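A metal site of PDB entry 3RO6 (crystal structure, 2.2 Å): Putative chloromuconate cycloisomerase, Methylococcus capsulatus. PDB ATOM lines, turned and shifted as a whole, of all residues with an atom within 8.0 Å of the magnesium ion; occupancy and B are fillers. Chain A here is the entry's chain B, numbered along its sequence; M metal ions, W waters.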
ATOM      1  N   LYS A 160     -17.729  -5.967 -16.230  1.00  0.00           N
ATOM      2  CA  LYS A 160     -17.836  -6.037 -17.693  1.00  0.00           C
ATOM      3  C   LYS A 160     -18.934  -7.036 -18.028  1.00  0.00           C
ATOM      4  O   LYS A 160     -18.810  -8.226 -17.738  1.00  0.00           O
ATOM      5  CB  LYS A 160     -16.509  -6.493 -18.305  1.00  0.00           C
ATOM      6  CG  LYS A 160     -16.497  -6.618 -19.829  1.00  0.00           C
ATOM      7  CD  LYS A 160     -15.126  -7.151 -20.272  1.00  0.00           C
ATOM      8  CE  LYS A 160     -15.130  -7.666 -21.691  1.00  0.00           C
ATOM      9  NZ  LYS A 160     -15.136  -6.547 -22.655  1.00  0.00           N
ATOM     10  N   LYS A 162     -21.316  -9.016 -20.688  1.00  0.00           N
ATOM     11  CA  LYS A 162     -21.555  -9.438 -22.071  1.00  0.00           C
ATOM     12  C   LYS A 162     -23.049  -9.366 -22.410  1.00  0.00           C
ATOM     13  O   LYS A 162     -23.910  -9.802 -21.628  1.00  0.00           O
ATOM     14  CB  LYS A 162     -21.027 -10.851 -22.308  1.00  0.00           C
ATOM     15  CG  LYS A 162     -19.564 -11.057 -22.021  1.00  0.00           C
ATOM     16  CD  LYS A 162     -19.072 -12.351 -22.666  1.00  0.00           C
ATOM     17  CE  LYS A 162     -17.622 -12.641 -22.306  1.00  0.00           C
ATOM     18  NZ  LYS A 162     -17.154 -13.944 -22.851  1.00  0.00           N
ATOM     19  N   VAL A 189     -20.026  -2.526 -21.171  1.00  0.00           N
ATOM     20  CA  VAL A 189     -20.724  -3.621 -21.851  1.00  0.00           C
ATOM     21  C   VAL A 189     -20.046  -4.107 -23.135  1.00  0.00           C
ATOM     22  O   VAL A 189     -19.358  -3.349 -23.823  1.00  0.00           O
ATOM     23  CB  VAL A 189     -22.221  -3.269 -22.118  1.00  0.00           C
ATOM     24  CG1 VAL A 189     -22.938  -2.941 -20.795  1.00  0.00           C
ATOM     25  CG2 VAL A 189     -22.331  -2.095 -23.113  1.00  0.00           C
ATOM     26  N   ASP A 190     -20.252  -5.379 -23.442  1.00  0.00           N
ATOM     27  CA  ASP A 190     -19.597  -6.001 -24.599  1.00  0.00           C
ATOM     28  C   ASP A 190     -20.564  -6.879 -25.387  1.00  0.00           C
ATOM     29  O   ASP A 190     -20.681  -8.076 -25.112  1.00  0.00           O
ATOM     30  CB  ASP A 190     -18.404  -6.835 -24.144  1.00  0.00           C
ATOM     31  CG  ASP A 190     -17.465  -7.191 -25.292  1.00  0.00           C
ATOM     32  OD1 ASP A 190     -17.912  -7.244 -26.461  1.00  0.00           O
ATOM     33  OD2 ASP A 190     -16.275  -7.436 -25.011  1.00  0.00           O
ATOM     34  N   PRO A 191     -21.290  -6.289 -26.339  1.00  0.00           N
ATOM     35  CA  PRO A 191     -22.191  -7.079 -27.196  1.00  0.00           C
ATOM     36  C   PRO A 191     -21.472  -7.993 -28.203  1.00  0.00           C
ATOM     37  O   PRO A 191     -22.092  -8.886 -28.795  1.00  0.00           O
ATOM     38  CB  PRO A 191     -23.041  -6.003 -27.888  1.00  0.00           C
ATOM     39  CG  PRO A 191     -22.250  -4.737 -27.769  1.00  0.00           C
ATOM     40  CD  PRO A 191     -21.478  -4.834 -26.511  1.00  0.00           C
ATOM     41  N   ASN A 192     -20.178  -7.759 -28.417  1.00  0.00           N
ATOM     42  CA  ASN A 192     -19.374  -8.535 -29.369  1.00  0.00           C
ATOM     43  C   ASN A 192     -20.069  -8.836 -30.705  1.00  0.00           C
ATOM     44  O   ASN A 192     -20.293  -9.985 -31.051  1.00  0.00           O
ATOM     45  CB  ASN A 192     -18.854  -9.839 -28.744  1.00  0.00           C
ATOM     46  CG  ASN A 192     -17.761 -10.501 -29.599  1.00  0.00           C
ATOM     47  OD1 ASN A 192     -17.196  -9.882 -30.503  1.00  0.00           O
ATOM     48  ND2 ASN A 192     -17.454 -11.750 -29.304  1.00  0.00           N
ATOM     49  N   GLN A 193     -20.364  -7.775 -31.462  1.00  0.00           N
ATOM     50  CA  GLN A 193     -20.769  -7.911 -32.869  1.00  0.00           C
ATOM     51  C   GLN A 193     -22.259  -8.174 -33.085  1.00  0.00           C
ATOM     52  O   GLN A 193     -22.721  -8.235 -34.211  1.00  0.00           O
ATOM     53  CB  GLN A 193     -19.885  -8.946 -33.597  1.00  0.00           C
ATOM     54  CG  GLN A 193     -18.413  -8.600 -33.465  1.00  0.00           C
ATOM     55  CD  GLN A 193     -17.493  -9.573 -34.177  1.00  0.00           C
ATOM     56  OE1 GLN A 193     -17.392  -9.565 -35.405  1.00  0.00           O
ATOM     57  NE2 GLN A 193     -16.805 -10.403 -33.405  1.00  0.00           N
ATOM     58  N   GLU A 216     -18.429  -1.854 -26.032  1.00  0.00           N
ATOM     59  CA  GLU A 216     -17.344  -2.446 -26.803  1.00  0.00           C
ATOM     60  C   GLU A 216     -17.885  -3.225 -27.995  1.00  0.00           C
ATOM     61  O   GLU A 216     -18.769  -4.078 -27.856  1.00  0.00           O
ATOM     62  CB  GLU A 216     -16.496  -3.344 -25.911  1.00  0.00           C
ATOM     63  CG  GLU A 216     -15.314  -3.927 -26.631  1.00  0.00           C
ATOM     64  CD  GLU A 216     -14.192  -4.296 -25.673  1.00  0.00           C
ATOM     65  OE1 GLU A 216     -13.453  -3.377 -25.250  1.00  0.00           O
ATOM     66  OE2 GLU A 216     -14.062  -5.480 -25.341  1.00  0.00           O
ATOM     67  N   GLN A 217     -17.358  -2.912 -29.184  1.00  0.00           N
ATOM     68  CA  GLN A 217     -17.590  -3.692 -30.410  1.00  0.00           C
ATOM     69  C   GLN A 217     -19.033  -4.104 -30.648  1.00  0.00           C
ATOM     70  O   GLN A 217     -19.341  -5.296 -30.701  1.00  0.00           O
ATOM     71  CB  GLN A 217     -16.688  -4.941 -30.439  1.00  0.00           C
ATOM     72  CG  GLN A 217     -16.569  -5.590 -31.848  1.00  0.00           C
ATOM     73  CD  GLN A 217     -15.698  -4.778 -32.828  1.00  0.00           C
ATOM     74  OE1 GLN A 217     -14.612  -4.322 -32.485  1.00  0.00           O
ATOM     75  NE2 GLN A 217     -16.188  -4.615 -34.063  1.00  0.00           N
ATOM     76  N   ALA A 239     -15.718   1.337 -28.088  1.00  0.00           N
ATOM     77  CA  ALA A 239     -14.379   0.780 -28.133  1.00  0.00           C
ATOM     78  C   ALA A 239     -14.282  -0.268 -29.231  1.00  0.00           C
ATOM     79  O   ALA A 239     -15.243  -0.989 -29.496  1.00  0.00           O
ATOM     80  CB  ALA A 239     -14.049   0.147 -26.804  1.00  0.00           C
ATOM     81  N   ALA A 240     -13.112  -0.337 -29.880  1.00  0.00           N
ATOM     82  CA  ALA A 240     -12.862  -1.310 -30.932  1.00  0.00           C
ATOM     83  C   ALA A 240     -12.161  -2.522 -30.348  1.00  0.00           C
ATOM     84  O   ALA A 240     -11.165  -2.395 -29.620  1.00  0.00           O
ATOM     85  CB  ALA A 240     -12.005  -0.677 -32.032  1.00  0.00           C
ATOM     86  N   ASP A 241     -12.684  -3.728 -30.601  1.00  0.00           N
ATOM     87  CA  ASP A 241     -11.973  -4.906 -30.107  1.00  0.00           C
ATOM     88  C   ASP A 241     -11.635  -5.894 -31.201  1.00  0.00           C
ATOM     89  O   ASP A 241     -10.498  -5.919 -31.703  1.00  0.00           O
ATOM     90  CB  ASP A 241     -12.749  -5.578 -28.958  1.00  0.00           C
ATOM     91  CG  ASP A 241     -12.069  -6.863 -28.442  1.00  0.00           C
ATOM     92  OD1 ASP A 241     -10.929  -7.168 -28.845  1.00  0.00           O
ATOM     93  OD2 ASP A 241     -12.689  -7.567 -27.605  1.00  0.00           O
ATOM     94  N   GLU A 242     -12.638  -6.655 -31.637  1.00  0.00           N
ATOM     95  CA  GLU A 242     -12.399  -7.613 -32.702  1.00  0.00           C
ATOM     96  C   GLU A 242     -12.012  -6.903 -34.007  1.00  0.00           C
ATOM     97  O   GLU A 242     -11.380  -7.493 -34.876  1.00  0.00           O
ATOM     98  CB  GLU A 242     -13.614  -8.531 -32.888  1.00  0.00           C
ATOM     99  CG  GLU A 242     -13.709  -9.667 -31.820  1.00  0.00           C
ATOM    100  CD  GLU A 242     -14.174  -9.191 -30.437  1.00  0.00           C
ATOM    101  OE1 GLU A 242     -14.819  -8.122 -30.319  1.00  0.00           O
ATOM    102  OE2 GLU A 242     -13.881  -9.898 -29.439  1.00  0.00           O
ATOM    103  N   ASN A 264      -9.076  -1.428 -27.809  1.00  0.00           N
ATOM    104  CA  ASN A 264      -8.833  -2.514 -26.880  1.00  0.00           C
ATOM    105  C   ASN A 264      -7.664  -3.357 -27.412  1.00  0.00           C
ATOM    106  O   ASN A 264      -7.779  -4.093 -28.394  1.00  0.00           O
ATOM    107  CB  ASN A 264     -10.119  -3.379 -26.702  1.00  0.00           C
ATOM    108  CG  ASN A 264      -9.896  -4.595 -25.788  1.00  0.00           C
ATOM    109  OD1 ASN A 264      -8.794  -5.117 -25.694  1.00  0.00           O
ATOM    110  ND2 ASN A 264     -10.957  -5.065 -25.138  1.00  0.00           N
ATOM    111  N   LYS A 266      -5.188  -6.397 -27.057  1.00  0.00           N
ATOM    112  CA  LYS A 266      -4.875  -7.698 -26.434  1.00  0.00           C
ATOM    113  C   LYS A 266      -3.598  -8.244 -27.042  1.00  0.00           C
ATOM    114  O   LYS A 266      -3.472  -8.276 -28.268  1.00  0.00           O
ATOM    115  CB  LYS A 266      -6.019  -8.690 -26.637  1.00  0.00           C
ATOM    116  CG  LYS A 266      -7.316  -8.259 -25.930  1.00  0.00           C
ATOM    117  CD  LYS A 266      -8.471  -9.209 -26.243  1.00  0.00           C
ATOM    118  CE  LYS A 266      -9.804  -8.531 -25.969  1.00  0.00           C
ATOM    119  NZ  LYS A 266     -10.946  -9.433 -26.293  1.00  0.00           N
ATOM    120  N   LYS A 269      -3.932 -10.642 -29.690  1.00  0.00           N
ATOM    121  CA  LYS A 269      -4.284 -10.066 -30.987  1.00  0.00           C
ATOM    122  C   LYS A 269      -3.159  -9.378 -31.772  1.00  0.00           C
ATOM    123  O   LYS A 269      -3.027  -9.612 -32.979  1.00  0.00           O
ATOM    124  CB  LYS A 269      -5.482  -9.116 -30.892  1.00  0.00           C
ATOM    125  CG  LYS A 269      -6.793  -9.777 -30.461  1.00  0.00           C
ATOM    126  CD  LYS A 269      -7.922  -8.756 -30.507  1.00  0.00           C
ATOM    127  CE  LYS A 269      -7.522  -7.499 -29.737  1.00  0.00           C
ATOM    128  NZ  LYS A 269      -8.550  -6.455 -29.824  1.00  0.00           N
ATOM    129  N   MET A 291      -7.496   0.569 -23.781  1.00  0.00           N
ATOM    130  CA  MET A 291      -8.093  -0.407 -22.909  1.00  0.00           C
ATOM    131  C   MET A 291      -7.237  -1.651 -23.133  1.00  0.00           C
ATOM    132  O   MET A 291      -6.844  -1.930 -24.261  1.00  0.00           O
ATOM    133  CB  MET A 291      -9.544  -0.595 -23.357  1.00  0.00           C
ATOM    134  CG  MET A 291     -10.139  -1.960 -23.191  1.00  0.00           C
ATOM    135  SD  MET A 291     -10.435  -2.357 -21.455  1.00  0.00           S
ATOM    136  CE  MET A 291      -9.850  -4.039 -21.525  1.00  0.00           C
ATOM    137  N   GLY A 293      -7.166  -5.666 -22.764  1.00  0.00           N
ATOM    138  CA  GLY A 293      -7.928  -6.858 -22.496  1.00  0.00           C
ATOM    139  C   GLY A 293      -7.044  -8.071 -22.521  1.00  0.00           C
ATOM    140  O   GLY A 293      -5.805  -7.952 -22.627  1.00  0.00           O
ATOM    141  N   CYS A 294      -7.672  -9.240 -22.487  1.00  0.00           N
ATOM    142  CA  CYS A 294      -6.943 -10.490 -22.462  1.00  0.00           C
ATOM    143  C   CYS A 294      -7.838 -11.663 -22.909  1.00  0.00           C
ATOM    144  O   CYS A 294      -9.036 -11.514 -23.111  1.00  0.00           O
ATOM    145  CB  CYS A 294      -6.474 -10.754 -21.027  1.00  0.00           C
ATOM    146  SG  CYS A 294      -7.891 -10.962 -19.858  1.00  0.00           S
ATOM    147  N   ASP A 319      -9.337  -4.709 -18.768  1.00  0.00           N
ATOM    148  CA  ASP A 319     -10.021  -5.951 -18.438  1.00  0.00           C
ATOM    149  C   ASP A 319      -8.936  -7.028 -18.443  1.00  0.00           C
ATOM    150  O   ASP A 319      -8.830  -7.860 -19.354  1.00  0.00           O
ATOM    151  CB  ASP A 319     -10.956  -6.333 -19.602  1.00  0.00           C
ATOM    152  CG  ASP A 319     -12.054  -5.287 -19.890  1.00  0.00           C
ATOM    153  OD1 ASP A 319     -12.515  -4.597 -18.967  1.00  0.00           O
ATOM    154  OD2 ASP A 319     -12.481  -5.198 -21.085  1.00  0.00           O
HETATM  155 MG    MG M   1     -14.458  -7.483 -26.311  1.00  0.00          MG
HETATM  156  O   HOH W   1     -13.452  -8.340 -24.447  1.00  0.00           O
HETATM  157  O   HOH W   2     -14.746  -9.552 -26.918  1.00  0.00           O
HETATM  158  O   HOH W   3     -15.726  -7.049 -28.136  1.00  0.00           O
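Water W3 lies within hydrogen-bond range of OE1 of Glu 242 (2.6 Å) and OD1 of Asp 190 (2.8 Å).
Water W1 bridges NZ of Lys 160 (3.0 Å) and NZ of Lys 266 (3.3 Å).
N of Glu 216 is in hydrogen-bond range of O of Val 189, at 2.8 Å.
The side-chain carboxylate of Asp 190 sits close to the side-chain amino group of Lys 160 (2.8 Å).
OD1 of Asn 192 sits close to OE1 of Glu 242 (3.0 Å).
The side-chain amino group of Lys 160 is in salt-bridge range of the side-chain carboxylate of Asp 319, at 3.4 Å.
The backbone NH (N) of Asn 192 sits at hydrogen-bond distance from the side-chain carboxylate (OD1) of Asp 190, at 3.0 Å.
The side-chain carboxylate (OD1) of Asp 241 is in salt-bridge range of the side-chain amino group (NZ) of Lys 269 (2.7 Å).
The side-chain carboxylate of Asp 241 is in salt-bridge range of the side-chain amino group of Lys 266 (3.4 Å).
The backbone NH (N) of Asp 241 sits at hydrogen-bond distance from the side-chain amide oxygen (OE1) of Gln 217 (2.8 Å).
Lys 160 touches the magnesium ion (NZ to MG, 3.8 Å).
Glu 242 touches the magnesium ion (OE2 to MG, 3.99 Å).
Within 4 Å of the magnesium ion: Lys 160, Asp 190, Glu 216, Asp 241 and Glu 242.
Along chain A the residues within 4 Å of the magnesium ion span positions 160 to 242.
The magnesium ion is bound by water W2 (2.2 Å), OD2 of Asp 241 (2.2 Å), OD2 of Asp 190 (2.2 Å), OE2 of Glu 216 (2.3 Å), water W3 (2.3 Å) and water W1 (2.3 Å).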
